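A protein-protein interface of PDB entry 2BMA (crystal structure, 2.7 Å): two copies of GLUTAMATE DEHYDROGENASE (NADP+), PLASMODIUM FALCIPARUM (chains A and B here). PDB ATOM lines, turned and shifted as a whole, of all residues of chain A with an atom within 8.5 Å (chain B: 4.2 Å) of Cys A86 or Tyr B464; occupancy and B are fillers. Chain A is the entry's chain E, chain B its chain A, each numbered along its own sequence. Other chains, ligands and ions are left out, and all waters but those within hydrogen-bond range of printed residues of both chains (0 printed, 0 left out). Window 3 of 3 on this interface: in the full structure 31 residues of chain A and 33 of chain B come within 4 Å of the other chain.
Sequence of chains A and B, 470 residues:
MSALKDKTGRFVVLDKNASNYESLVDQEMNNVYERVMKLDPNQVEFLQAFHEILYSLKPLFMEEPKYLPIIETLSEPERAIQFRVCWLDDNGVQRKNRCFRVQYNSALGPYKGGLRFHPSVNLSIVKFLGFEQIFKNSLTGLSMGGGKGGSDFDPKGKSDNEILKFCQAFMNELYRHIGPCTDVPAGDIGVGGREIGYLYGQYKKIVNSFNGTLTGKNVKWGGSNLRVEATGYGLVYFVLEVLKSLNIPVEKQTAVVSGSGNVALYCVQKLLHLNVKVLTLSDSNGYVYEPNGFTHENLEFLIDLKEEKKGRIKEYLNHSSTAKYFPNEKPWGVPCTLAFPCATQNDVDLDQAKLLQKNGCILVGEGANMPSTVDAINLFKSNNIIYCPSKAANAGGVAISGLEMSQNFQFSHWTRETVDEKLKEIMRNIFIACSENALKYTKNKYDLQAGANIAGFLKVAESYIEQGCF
The side-chain sulfur (SG) of Cys A86 sits close to the backbone carbonyl oxygen (O) of Arg A95. The backbone carbonyl oxygen (O) of Trp A87 lies within hydrogen-bond range of the backbone NH (N) of Arg A95, at 2.7 Å. The indole nitrogen (NE1) of Trp A87 sits at hydrogen-bond distance from the side-chain amide oxygen (OD1) of Asn A97 (3.0 Å).
Hydrophobic or aromatic side chains of chain B within 4 Å of the printed part of chain A: Tyr B464. Printed residues of chain A that touch a printed residue of chain B: Arg A84, Cys A86, Trp A87, Gln A94 and Lys A96. Along chain A the printed residues that touch a printed residue of chain B span positions 84 to 96. Among the printed residues, 12 pairs touch across the chains.
Arg A84 touches Leu B74 (NH1 to CA, 3.9 Å). NH2 of Arg A84 touches CE1 of Tyr B464 (3.5 Å). Thr B73 touches Cys A86. N of Cys A86 touches O of Phe B470 (3.8 Å). Lys A96 touches Thr B73 (CD to CA, 3.9 Å).
Cys A86 touches just these residues of chain B: Thr B73 (3.9 Å), Tyr B464 (3.5 Å), Cys B469 (3.4 Å) and Phe B470 (3.8 Å). Gln A168 touches none of the printed residues of chain B. Of the printed residues of chain A, Leu B74 touches Arg A84. No residue of chain A comes within 4 Å of Ser B463. Tyr B464 touches three residues of chain A. Printed residues of chain A within 4 Å of Cys B469: Cys A86 (3.4 Å), Trp A87 (3.6 Å) and Gln A94 (3.2 Å). The nearest printed residue of chain B that does not touch Trp A87 is Phe B470 (6.4 Å).
NH1 of Arg A84 lies close to O of Thr B73 (3.4 Å). OH of Tyr B464 is in hydrogen-bond range of SG of Cys A86. The side-chain amide nitrogen (NE2) of Gln A94 lies within hydrogen-bond range of the side-chain hydroxyl (OH) of Tyr B464, 2.8 Å away. The side-chain sulfur (SG) of Cys B469 sits close to the backbone carbonyl oxygen (O) of Cys A86. The side-chain sulfur (SG) of Cys B469 is in hydrogen-bond range of the backbone NH (N) of Trp A87 (3.6 Å). The side-chain sulfur (SG) of Cys B469 sits close to the side-chain amide oxygen (OE1) of Gln A94 (3.6 Å). The guanidinium group (NH2) of Arg A84 is in salt-bridge range of the chain-end carboxylate (OXT) of Phe B470, 3.4 Å away.
No position is printed for both chains. Of the 12 pairs that touch across the chains among the printed residues, none has its exchanged pair printed and touching as well.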
ATOM      1  N   PHE A  83       3.319   3.061 -13.670  1.00  0.00           N
ATOM      2  CA  PHE A  83       3.191   2.711 -12.259  1.00  0.00           C
ATOM      3  C   PHE A  83       3.688   1.337 -11.857  1.00  0.00           C
ATOM      4  O   PHE A  83       3.719   0.408 -12.654  1.00  0.00           O
ATOM      5  CB  PHE A  83       1.739   2.880 -11.791  1.00  0.00           C
ATOM      6  CG  PHE A  83       0.719   2.086 -12.582  1.00  0.00           C
ATOM      7  CD1 PHE A  83       0.005   1.050 -11.981  1.00  0.00           C
ATOM      8  CD2 PHE A  83       0.420   2.418 -13.902  1.00  0.00           C
ATOM      9  CE1 PHE A  83      -0.996   0.361 -12.681  1.00  0.00           C
ATOM     10  CE2 PHE A  83      -0.571   1.739 -14.602  1.00  0.00           C
ATOM     11  CZ  PHE A  83      -1.281   0.709 -13.988  1.00  0.00           C
ATOM     12  N   ARG A  84       4.088   1.229 -10.598  1.00  0.00           N
ATOM     13  CA  ARG A  84       4.581  -0.021 -10.025  1.00  0.00           C
ATOM     14  C   ARG A  84       3.386  -0.805  -9.501  1.00  0.00           C
ATOM     15  O   ARG A  84       2.423  -0.231  -9.002  1.00  0.00           O
ATOM     16  CB  ARG A  84       5.548   0.278  -8.872  1.00  0.00           C
ATOM     17  CG  ARG A  84       6.282  -0.929  -8.288  1.00  0.00           C
ATOM     18  CD  ARG A  84       7.317  -0.471  -7.248  1.00  0.00           C
ATOM     19  NE  ARG A  84       6.733  -0.245  -5.920  1.00  0.00           N
ATOM     20  CZ  ARG A  84       7.203   0.627  -5.031  1.00  0.00           C
ATOM     21  NH1 ARG A  84       8.266   1.366  -5.331  1.00  0.00           N
ATOM     22  NH2 ARG A  84       6.622   0.755  -3.840  1.00  0.00           N
ATOM     23  N   VAL A  85       3.450  -2.118  -9.623  1.00  0.00           N
ATOM     24  CA  VAL A  85       2.368  -2.957  -9.153  1.00  0.00           C
ATOM     25  C   VAL A  85       2.924  -4.210  -8.504  1.00  0.00           C
ATOM     26  O   VAL A  85       3.607  -4.997  -9.153  1.00  0.00           O
ATOM     27  CB  VAL A  85       1.443  -3.346 -10.312  1.00  0.00           C
ATOM     28  CG1 VAL A  85       0.551  -4.494  -9.908  1.00  0.00           C
ATOM     29  CG2 VAL A  85       0.599  -2.143 -10.708  1.00  0.00           C
ATOM     30  N   CYS A  86       2.631  -4.379  -7.219  1.00  0.00           N
ATOM     31  CA  CYS A  86       3.088  -5.527  -6.455  1.00  0.00           C
ATOM     32  C   CYS A  86       1.926  -6.466  -6.165  1.00  0.00           C
ATOM     33  O   CYS A  86       0.818  -6.007  -5.909  1.00  0.00           O
ATOM     34  CB  CYS A  86       3.715  -5.053  -5.142  1.00  0.00           C
ATOM     35  SG  CYS A  86       5.244  -4.121  -5.398  1.00  0.00           S
ATOM     36  N   TRP A  87       2.182  -7.773  -6.196  1.00  0.00           N
ATOM     37  CA  TRP A  87       1.151  -8.786  -5.929  1.00  0.00           C
ATOM     38  C   TRP A  87       1.776 -10.095  -5.412  1.00  0.00           C
ATOM     39  O   TRP A  87       2.916 -10.413  -5.737  1.00  0.00           O
ATOM     40  CB  TRP A  87       0.355  -9.075  -7.198  1.00  0.00           C
ATOM     41  CG  TRP A  87       1.239  -9.485  -8.318  1.00  0.00           C
ATOM     42  CD1 TRP A  87       2.080  -8.683  -9.029  1.00  0.00           C
ATOM     43  CD2 TRP A  87       1.434 -10.815  -8.811  1.00  0.00           C
ATOM     44  NE1 TRP A  87       2.791  -9.432  -9.933  1.00  0.00           N
ATOM     45  CE2 TRP A  87       2.413 -10.744  -9.823  1.00  0.00           C
ATOM     46  CE3 TRP A  87       0.876 -12.061  -8.496  1.00  0.00           C
ATOM     47  CZ2 TRP A  87       2.852 -11.871 -10.523  1.00  0.00           C
ATOM     48  CZ3 TRP A  87       1.313 -13.182  -9.191  1.00  0.00           C
ATOM     49  CH2 TRP A  87       2.293 -13.079 -10.194  1.00  0.00           C
ATOM     50  N   LEU A  88       1.025 -10.848  -4.613  1.00  0.00           N
ATOM     51  CA  LEU A  88       1.519 -12.094  -4.055  1.00  0.00           C
ATOM     52  C   LEU A  88       1.285 -13.271  -4.995  1.00  0.00           C
ATOM     53  O   LEU A  88       0.159 -13.489  -5.457  1.00  0.00           O
ATOM     54  CB  LEU A  88       0.819 -12.392  -2.728  1.00  0.00           C
ATOM     55  CG  LEU A  88       0.838 -11.347  -1.613  1.00  0.00           C
ATOM     56  CD1 LEU A  88       0.008 -11.835  -0.447  1.00  0.00           C
ATOM     57  CD2 LEU A  88       2.254 -11.090  -1.177  1.00  0.00           C
ATOM     58  N   ASP A  89       2.336 -14.037  -5.287  1.00  0.00           N
ATOM     59  CA  ASP A  89       2.159 -15.197  -6.147  1.00  0.00           C
ATOM     60  C   ASP A  89       1.600 -16.302  -5.277  1.00  0.00           C
ATOM     61  O   ASP A  89       1.493 -16.148  -4.059  1.00  0.00           O
ATOM     62  CB  ASP A  89       3.474 -15.616  -6.854  1.00  0.00           C
ATOM     63  CG  ASP A  89       4.599 -15.996  -5.896  1.00  0.00           C
ATOM     64  OD1 ASP A  89       5.763 -15.670  -6.210  1.00  0.00           O
ATOM     65  OD2 ASP A  89       4.349 -16.636  -4.856  1.00  0.00           O
ATOM     66  N   VAL A  93       5.287 -15.367  -2.139  1.00  0.00           N
ATOM     67  CA  VAL A  93       6.361 -14.456  -2.502  1.00  0.00           C
ATOM     68  C   VAL A  93       5.774 -13.206  -3.137  1.00  0.00           C
ATOM     69  O   VAL A  93       4.958 -13.302  -4.047  1.00  0.00           O
ATOM     70  CB  VAL A  93       7.346 -15.117  -3.512  1.00  0.00           C
ATOM     71  CG1 VAL A  93       8.319 -14.076  -4.065  1.00  0.00           C
ATOM     72  CG2 VAL A  93       8.134 -16.226  -2.824  1.00  0.00           C
ATOM     73  N   GLN A  94       6.181 -12.042  -2.646  1.00  0.00           N
ATOM     74  CA  GLN A  94       5.705 -10.774  -3.188  1.00  0.00           C
ATOM     75  C   GLN A  94       6.330 -10.573  -4.570  1.00  0.00           C
ATOM     76  O   GLN A  94       7.508 -10.828  -4.750  1.00  0.00           O
ATOM     77  CB  GLN A  94       6.114  -9.637  -2.250  1.00  0.00           C
ATOM     78  CG  GLN A  94       5.715  -8.261  -2.728  1.00  0.00           C
ATOM     79  CD  GLN A  94       5.773  -7.223  -1.626  1.00  0.00           C
ATOM     80  OE1 GLN A  94       5.217  -7.426  -0.539  1.00  0.00           O
ATOM     81  NE2 GLN A  94       6.433  -6.098  -1.901  1.00  0.00           N
ATOM     82  N   ARG A  95       5.550 -10.120  -5.540  1.00  0.00           N
ATOM     83  CA  ARG A  95       6.068  -9.897  -6.896  1.00  0.00           C
ATOM     84  C   ARG A  95       5.958  -8.432  -7.374  1.00  0.00           C
ATOM     85  O   ARG A  95       5.257  -7.621  -6.772  1.00  0.00           O
ATOM     86  CB  ARG A  95       5.337 -10.809  -7.880  1.00  0.00           C
ATOM     87  CG  ARG A  95       5.440 -12.291  -7.577  1.00  0.00           C
ATOM     88  CD  ARG A  95       6.800 -12.880  -7.965  1.00  0.00           C
ATOM     89  NE  ARG A  95       6.633 -14.176  -8.621  1.00  0.00           N
ATOM     90  CZ  ARG A  95       6.483 -14.332  -9.937  1.00  0.00           C
ATOM     91  NH1 ARG A  95       6.504 -13.272 -10.741  1.00  0.00           N
ATOM     92  NH2 ARG A  95       6.254 -15.543 -10.446  1.00  0.00           N
ATOM     93  N   LYS A  96       6.644  -8.106  -8.467  1.00  0.00           N
ATOM     94  CA  LYS A  96       6.641  -6.739  -8.996  1.00  0.00           C
ATOM     95  C   LYS A  96       6.561  -6.682 -10.525  1.00  0.00           C
ATOM     96  O   LYS A  96       7.248  -7.437 -11.216  1.00  0.00           O
ATOM     97  CB  LYS A  96       7.909  -6.004  -8.549  1.00  0.00           C
ATOM     98  CG  LYS A  96       7.956  -4.540  -8.960  1.00  0.00           C
ATOM     99  CD  LYS A  96       9.381  -4.069  -9.264  1.00  0.00           C
ATOM    100  CE  LYS A  96       9.813  -4.436 -10.692  1.00  0.00           C
ATOM    101  NZ  LYS A  96       9.024  -3.751 -11.756  1.00  0.00           N
ATOM    102  N   ASN A  97       5.731  -5.774 -11.043  1.00  0.00           N
ATOM    103  CA  ASN A  97       5.565  -5.595 -12.488  1.00  0.00           C
ATOM    104  C   ASN A  97       5.468  -4.122 -12.856  1.00  0.00           C
ATOM    105  O   ASN A  97       4.972  -3.318 -12.084  1.00  0.00           O
ATOM    106  CB  ASN A  97       4.301  -6.296 -12.990  1.00  0.00           C
ATOM    107  CG  ASN A  97       4.505  -7.771 -13.258  1.00  0.00           C
ATOM    108  OD1 ASN A  97       4.360  -8.613 -12.372  1.00  0.00           O
ATOM    109  ND2 ASN A  97       4.843  -8.093 -14.494  1.00  0.00           N
ATOM    110  N   ARG A  98       5.944  -3.773 -14.040  1.00  0.00           N
ATOM    111  CA  ARG A  98       5.881  -2.390 -14.502  1.00  0.00           C
ATOM    112  C   ARG A  98       4.615  -2.240 -15.338  1.00  0.00           C
ATOM    113  O   ARG A  98       4.345  -3.047 -16.230  1.00  0.00           O
ATOM    114  CB  ARG A  98       7.117  -2.039 -15.337  1.00  0.00           C
ATOM    115  CG  ARG A  98       7.003  -0.736 -16.116  1.00  0.00           C
ATOM    116  CD  ARG A  98       8.321  -0.388 -16.790  1.00  0.00           C
ATOM    117  NE  ARG A  98       9.348  -0.044 -15.810  1.00  0.00           N
ATOM    118  CZ  ARG A  98      10.544   0.449 -16.117  1.00  0.00           C
ATOM    119  NH1 ARG A  98      10.871   0.650 -17.386  1.00  0.00           N
ATOM    120  NH2 ARG A  98      11.406   0.771 -15.160  1.00  0.00           N
ATOM    121  N   CYS A  99       3.842  -1.204 -15.052  1.00  0.00           N
ATOM    122  CA  CYS A  99       2.597  -1.002 -15.767  1.00  0.00           C
ATOM    123  C   CYS A  99       2.501   0.352 -16.449  1.00  0.00           C
ATOM    124  O   CYS A  99       3.191   1.302 -16.089  1.00  0.00           O
ATOM    125  CB  CYS A  99       1.441  -1.188 -14.794  1.00  0.00           C
ATOM    126  SG  CYS A  99       1.633  -2.675 -13.798  1.00  0.00           S
ATOM    127  N   LYS A 165      -5.222 -11.574  -8.503  1.00  0.00           N
ATOM    128  CA  LYS A 165      -4.479 -10.719  -7.592  1.00  0.00           C
ATOM    129  C   LYS A 165      -3.743  -9.664  -8.374  1.00  0.00           C
ATOM    130  O   LYS A 165      -3.651  -8.518  -7.945  1.00  0.00           O
ATOM    131  CB  LYS A 165      -3.465 -11.520  -6.782  1.00  0.00           C
ATOM    132  CG  LYS A 165      -4.039 -12.626  -5.895  1.00  0.00           C
ATOM    133  CD  LYS A 165      -2.892 -13.381  -5.262  1.00  0.00           C
ATOM    134  CE  LYS A 165      -3.319 -14.734  -4.755  1.00  0.00           C
ATOM    135  NZ  LYS A 165      -2.134 -15.604  -4.496  1.00  0.00           N
ATOM    136  N   PHE A 166      -3.197 -10.030  -9.524  1.00  0.00           N
ATOM    137  CA  PHE A 166      -2.499  -9.017 -10.292  1.00  0.00           C
ATOM    138  C   PHE A 166      -3.504  -8.048 -10.878  1.00  0.00           C
ATOM    139  O   PHE A 166      -3.217  -6.867 -10.999  1.00  0.00           O
ATOM    140  CB  PHE A 166      -1.681  -9.595 -11.438  1.00  0.00           C
ATOM    141  CG  PHE A 166      -1.002  -8.533 -12.254  1.00  0.00           C
ATOM    142  CD1 PHE A 166       0.161  -7.935 -11.803  1.00  0.00           C
ATOM    143  CD2 PHE A 166      -1.574  -8.067 -13.431  1.00  0.00           C
ATOM    144  CE1 PHE A 166       0.742  -6.891 -12.506  1.00  0.00           C
ATOM    145  CE2 PHE A 166      -0.991  -7.017 -14.140  1.00  0.00           C
ATOM    146  CZ  PHE A 166       0.165  -6.434 -13.675  1.00  0.00           C
ATOM    147  N   CYS A 167      -4.674  -8.550 -11.259  1.00  0.00           N
ATOM    148  CA  CYS A 167      -5.702  -7.695 -11.829  1.00  0.00           C
ATOM    149  C   CYS A 167      -6.269  -6.713 -10.819  1.00  0.00           C
ATOM    150  O   CYS A 167      -6.657  -5.600 -11.179  1.00  0.00           O
ATOM    151  CB  CYS A 167      -6.826  -8.534 -12.422  1.00  0.00           C
ATOM    152  SG  CYS A 167      -6.584  -8.878 -14.172  1.00  0.00           S
ATOM    153  N   GLN A 168      -6.313  -7.122  -9.555  1.00  0.00           N
ATOM    154  CA  GLN A 168      -6.825  -6.257  -8.499  1.00  0.00           C
ATOM    155  C   GLN A 168      -5.773  -5.233  -8.108  1.00  0.00           C
ATOM    156  O   GLN A 168      -6.093  -4.098  -7.743  1.00  0.00           O
ATOM    157  CB  GLN A 168      -7.225  -7.087  -7.280  1.00  0.00           C
ATOM    158  CG  GLN A 168      -8.207  -8.181  -7.598  1.00  0.00           C
ATOM    159  CD  GLN A 168      -8.850  -8.743  -6.366  1.00  0.00           C
ATOM    160  OE1 GLN A 168      -8.180  -9.013  -5.374  1.00  0.00           O
ATOM    161  NE2 GLN A 168     -10.159  -8.936  -6.422  1.00  0.00           N
ATOM    162  N   ALA A 169      -4.514  -5.645  -8.183  1.00  0.00           N
ATOM    163  CA  ALA A 169      -3.395  -4.773  -7.844  1.00  0.00           C
ATOM    164  C   ALA A 169      -3.249  -3.690  -8.904  1.00  0.00           C
ATOM    165  O   ALA A 169      -3.053  -2.521  -8.574  1.00  0.00           O
ATOM    166  CB  ALA A 169      -2.117  -5.587  -7.747  1.00  0.00           C
ATOM    167  N   PHE A 170      -3.356  -4.094 -10.170  1.00  0.00           N
ATOM    168  CA  PHE A 170      -3.246  -3.196 -11.305  1.00  0.00           C
ATOM    169  C   PHE A 170      -4.287  -2.089 -11.185  1.00  0.00           C
ATOM    170  O   PHE A 170      -3.957  -0.908 -11.251  1.00  0.00           O
ATOM    171  CB  PHE A 170      -3.474  -3.979 -12.592  1.00  0.00           C
ATOM    172  CG  PHE A 170      -3.214  -3.199 -13.843  1.00  0.00           C
ATOM    173  CD1 PHE A 170      -1.933  -3.117 -14.372  1.00  0.00           C
ATOM    174  CD2 PHE A 170      -4.260  -2.586 -14.523  1.00  0.00           C
ATOM    175  CE1 PHE A 170      -1.702  -2.439 -15.571  1.00  0.00           C
ATOM    176  CE2 PHE A 170      -4.036  -1.908 -15.716  1.00  0.00           C
ATOM    177  CZ  PHE A 170      -2.758  -1.837 -16.241  1.00  0.00           C
ATOM    178  N   ASN A 172      -5.852  -1.244  -8.594  1.00  0.00           N
ATOM    179  CA  ASN A 172      -5.684  -0.542  -7.335  1.00  0.00           C
ATOM    180  C   ASN A 172      -4.950   0.768  -7.526  1.00  0.00           C
ATOM    181  O   ASN A 172      -4.881   1.576  -6.616  1.00  0.00           O
ATOM    182  CB  ASN A 172      -4.934  -1.424  -6.335  1.00  0.00           C
ATOM    183  CG  ASN A 172      -5.865  -2.268  -5.499  1.00  0.00           C
ATOM    184  OD1 ASN A 172      -5.443  -3.183  -4.806  1.00  0.00           O
ATOM    185  ND2 ASN A 172      -7.138  -1.954  -5.552  1.00  0.00           N
ATOM    186  N   GLU A 173      -4.389   0.965  -8.708  1.00  0.00           N
ATOM    187  CA  GLU A 173      -3.672   2.191  -9.023  1.00  0.00           C
ATOM    188  C   GLU A 173      -4.334   2.859 -10.216  1.00  0.00           C
ATOM    189  O   GLU A 173      -4.589   4.061 -10.196  1.00  0.00           O
ATOM    190  CB  GLU A 173      -2.199   1.908  -9.355  1.00  0.00           C
ATOM    191  CG  GLU A 173      -1.471   3.102  -9.979  1.00  0.00           C
ATOM    192  CD  GLU A 173      -1.542   4.377  -9.129  1.00  0.00           C
ATOM    193  OE1 GLU A 173      -1.397   5.475  -9.714  1.00  0.00           O
ATOM    194  OE2 GLU A 173      -1.729   4.298  -7.890  1.00  0.00           O
ATOM    195  N   THR B  73      12.840  -3.492  -5.989  1.00  0.00           N
ATOM    196  CA  THR B  73      11.460  -3.035  -6.142  1.00  0.00           C
ATOM    197  C   THR B  73      11.313  -1.527  -5.957  1.00  0.00           C
ATOM    198  O   THR B  73      10.513  -0.894  -6.633  1.00  0.00           O
ATOM    199  CB  THR B  73      10.535  -3.730  -5.133  1.00  0.00           C
ATOM    200  OG1 THR B  73      10.638  -5.148  -5.293  1.00  0.00           O
ATOM    201  CG2 THR B  73       9.090  -3.307  -5.355  1.00  0.00           C
ATOM    202  N   LEU B  74      12.079  -0.962  -5.029  1.00  0.00           N
ATOM    203  CA  LEU B  74      12.032   0.468  -4.757  1.00  0.00           C
ATOM    204  C   LEU B  74      12.727   1.277  -5.853  1.00  0.00           C
ATOM    205  O   LEU B  74      12.573   2.491  -5.918  1.00  0.00           O
ATOM    206  CB  LEU B  74      12.682   0.765  -3.395  1.00  0.00           C
ATOM    207  CG  LEU B  74      12.152  -0.023  -2.181  1.00  0.00           C
ATOM    208  CD1 LEU B  74      12.929   0.367  -0.933  1.00  0.00           C
ATOM    209  CD2 LEU B  74      10.674   0.241  -1.977  1.00  0.00           C
ATOM    210  N   VAL B 460      13.543   3.486   5.190  1.00  0.00           N
ATOM    211  CA  VAL B 460      12.659   3.313   4.062  1.00  0.00           C
ATOM    212  C   VAL B 460      12.235   1.855   3.913  1.00  0.00           C
ATOM    213  O   VAL B 460      11.042   1.540   3.953  1.00  0.00           O
ATOM    214  CB  VAL B 460      13.357   3.797   2.790  1.00  0.00           C
ATOM    215  CG1 VAL B 460      12.570   3.378   1.556  1.00  0.00           C
ATOM    216  CG2 VAL B 460      13.523   5.312   2.863  1.00  0.00           C
ATOM    217  N   ALA B 461      13.223   0.971   3.762  1.00  0.00           N
ATOM    218  CA  ALA B 461      12.983  -0.461   3.579  1.00  0.00           C
ATOM    219  C   ALA B 461      12.176  -1.148   4.696  1.00  0.00           C
ATOM    220  O   ALA B 461      11.286  -1.953   4.414  1.00  0.00           O
ATOM    221  CB  ALA B 461      14.310  -1.182   3.370  1.00  0.00           C
ATOM    222  N   GLU B 462      12.497  -0.857   5.953  1.00  0.00           N
ATOM    223  CA  GLU B 462      11.751  -1.453   7.052  1.00  0.00           C
ATOM    224  C   GLU B 462      10.309  -0.981   6.890  1.00  0.00           C
ATOM    225  O   GLU B 462       9.400  -1.798   6.783  1.00  0.00           O
ATOM    226  CB  GLU B 462      12.294  -0.991   8.414  1.00  0.00           C
ATOM    227  CG  GLU B 462      13.728  -1.412   8.732  1.00  0.00           C
ATOM    228  CD  GLU B 462      14.276  -0.749  10.014  1.00  0.00           C
ATOM    229  OE1 GLU B 462      13.701  -0.962  11.119  1.00  0.00           O
ATOM    230  OE2 GLU B 462      15.286  -0.008   9.914  1.00  0.00           O
ATOM    231  N   SER B 463      10.114   0.339   6.865  1.00  0.00           N
ATOM    232  CA  SER B 463       8.787   0.939   6.699  1.00  0.00           C
ATOM    233  C   SER B 463       8.013   0.269   5.565  1.00  0.00           C
ATOM    234  O   SER B 463       6.849  -0.114   5.732  1.00  0.00           O
ATOM    235  CB  SER B 463       8.901   2.442   6.403  1.00  0.00           C
ATOM    236  OG  SER B 463       9.285   3.180   7.556  1.00  0.00           O
ATOM    237  N   TYR B 464       8.657   0.140   4.406  1.00  0.00           N
ATOM    238  CA  TYR B 464       8.017  -0.496   3.265  1.00  0.00           C
ATOM    239  C   TYR B 464       7.482  -1.872   3.671  1.00  0.00           C
ATOM    240  O   TYR B 464       6.305  -2.176   3.461  1.00  0.00           O
ATOM    241  CB  TYR B 464       9.010  -0.646   2.120  1.00  0.00           C
ATOM    242  CG  TYR B 464       8.438  -1.362   0.926  1.00  0.00           C
ATOM    243  CD1 TYR B 464       7.564  -0.715   0.045  1.00  0.00           C
ATOM    244  CD2 TYR B 464       8.758  -2.690   0.683  1.00  0.00           C
ATOM    245  CE1 TYR B 464       7.023  -1.376  -1.056  1.00  0.00           C
ATOM    246  CE2 TYR B 464       8.229  -3.368  -0.405  1.00  0.00           C
ATOM    247  CZ  TYR B 464       7.362  -2.711  -1.275  1.00  0.00           C
ATOM    248  OH  TYR B 464       6.847  -3.399  -2.350  1.00  0.00           O
ATOM    249  N   ILE B 465       8.344  -2.691   4.261  1.00  0.00           N
ATOM    250  CA  ILE B 465       7.966  -4.032   4.699  1.00  0.00           C
ATOM    251  C   ILE B 465       6.788  -3.958   5.664  1.00  0.00           C
ATOM    252  O   ILE B 465       5.829  -4.728   5.568  1.00  0.00           O
ATOM    253  CB  ILE B 465       9.150  -4.759   5.416  1.00  0.00           C
ATOM    254  CG1 ILE B 465      10.390  -4.759   4.519  1.00  0.00           C
ATOM    255  CG2 ILE B 465       8.780  -6.210   5.715  1.00  0.00           C
ATOM    256  CD1 ILE B 465      11.652  -5.150   5.236  1.00  0.00           C
ATOM    257  N   GLU B 466       6.867  -3.022   6.597  1.00  0.00           N
ATOM    258  CA  GLU B 466       5.805  -2.860   7.577  1.00  0.00           C
ATOM    259  C   GLU B 466       4.499  -2.406   6.926  1.00  0.00           C
ATOM    260  O   GLU B 466       3.415  -2.769   7.386  1.00  0.00           O
ATOM    261  CB  GLU B 466       6.227  -1.863   8.668  1.00  0.00           C
ATOM    262  CG  GLU B 466       7.395  -2.337   9.507  1.00  0.00           C
ATOM    263  CD  GLU B 466       7.935  -1.258  10.425  1.00  0.00           C
ATOM    264  OE1 GLU B 466       8.844  -1.565  11.227  1.00  0.00           O
ATOM    265  OE2 GLU B 466       7.456  -0.100  10.347  1.00  0.00           O
ATOM    266  N   GLN B 467       4.600  -1.634   5.849  1.00  0.00           N
ATOM    267  CA  GLN B 467       3.407  -1.133   5.184  1.00  0.00           C
ATOM    268  C   GLN B 467       2.685  -2.146   4.292  1.00  0.00           C
ATOM    269  O   GLN B 467       1.501  -1.967   3.994  1.00  0.00           O
ATOM    270  CB  GLN B 467       3.746   0.169   4.451  1.00  0.00           C
ATOM    271  CG  GLN B 467       3.927   1.312   5.457  1.00  0.00           C
ATOM    272  CD  GLN B 467       4.267   2.652   4.842  1.00  0.00           C
ATOM    273  OE1 GLN B 467       3.934   2.925   3.690  1.00  0.00           O
ATOM    274  NE2 GLN B 467       4.911   3.512   5.628  1.00  0.00           N
ATOM    275  N   GLY B 468       3.379  -3.212   3.889  1.00  0.00           N
ATOM    276  CA  GLY B 468       2.739  -4.249   3.095  1.00  0.00           C
ATOM    277  C   GLY B 468       2.996  -4.243   1.608  1.00  0.00           C
ATOM    278  O   GLY B 468       3.758  -3.416   1.094  1.00  0.00           O
ATOM    279  N   CYS B 469       2.342  -5.165   0.907  1.00  0.00           N
ATOM    280  CA  CYS B 469       2.509  -5.282  -0.534  1.00  0.00           C
ATOM    281  C   CYS B 469       1.733  -4.235  -1.346  1.00  0.00           C
ATOM    282  O   CYS B 469       0.545  -4.401  -1.623  1.00  0.00           O
ATOM    283  CB  CYS B 469       2.112  -6.694  -0.978  1.00  0.00           C
ATOM    284  SG  CYS B 469       2.423  -7.062  -2.720  1.00  0.00           S
ATOM    285  N   PHE B 470       2.423  -3.157  -1.726  1.00  0.00           N
ATOM    286  CA  PHE B 470       1.823  -2.085  -2.525  1.00  0.00           C
ATOM    287  C   PHE B 470       2.791  -1.555  -3.574  1.00  0.00           C
ATOM    288  O   PHE B 470       2.393  -1.532  -4.767  1.00  0.00           O
ATOM    289  CB  PHE B 470       1.374  -0.914  -1.644  1.00  0.00           C
ATOM    290  CG  PHE B 470       2.499  -0.206  -0.931  1.00  0.00           C
ATOM    291  CD1 PHE B 470       3.029  -0.724   0.253  1.00  0.00           C
ATOM    292  CD2 PHE B 470       2.999   1.003  -1.420  1.00  0.00           C
ATOM    293  CE1 PHE B 470       4.040  -0.042   0.945  1.00  0.00           C
ATOM    294  CE2 PHE B 470       4.011   1.691  -0.733  1.00  0.00           C
ATOM    295  CZ  PHE B 470       4.530   1.170   0.450  1.00  0.00           C
ATOM    296  OXT PHE B 470       3.924  -1.167  -3.180  1.00  0.00           O
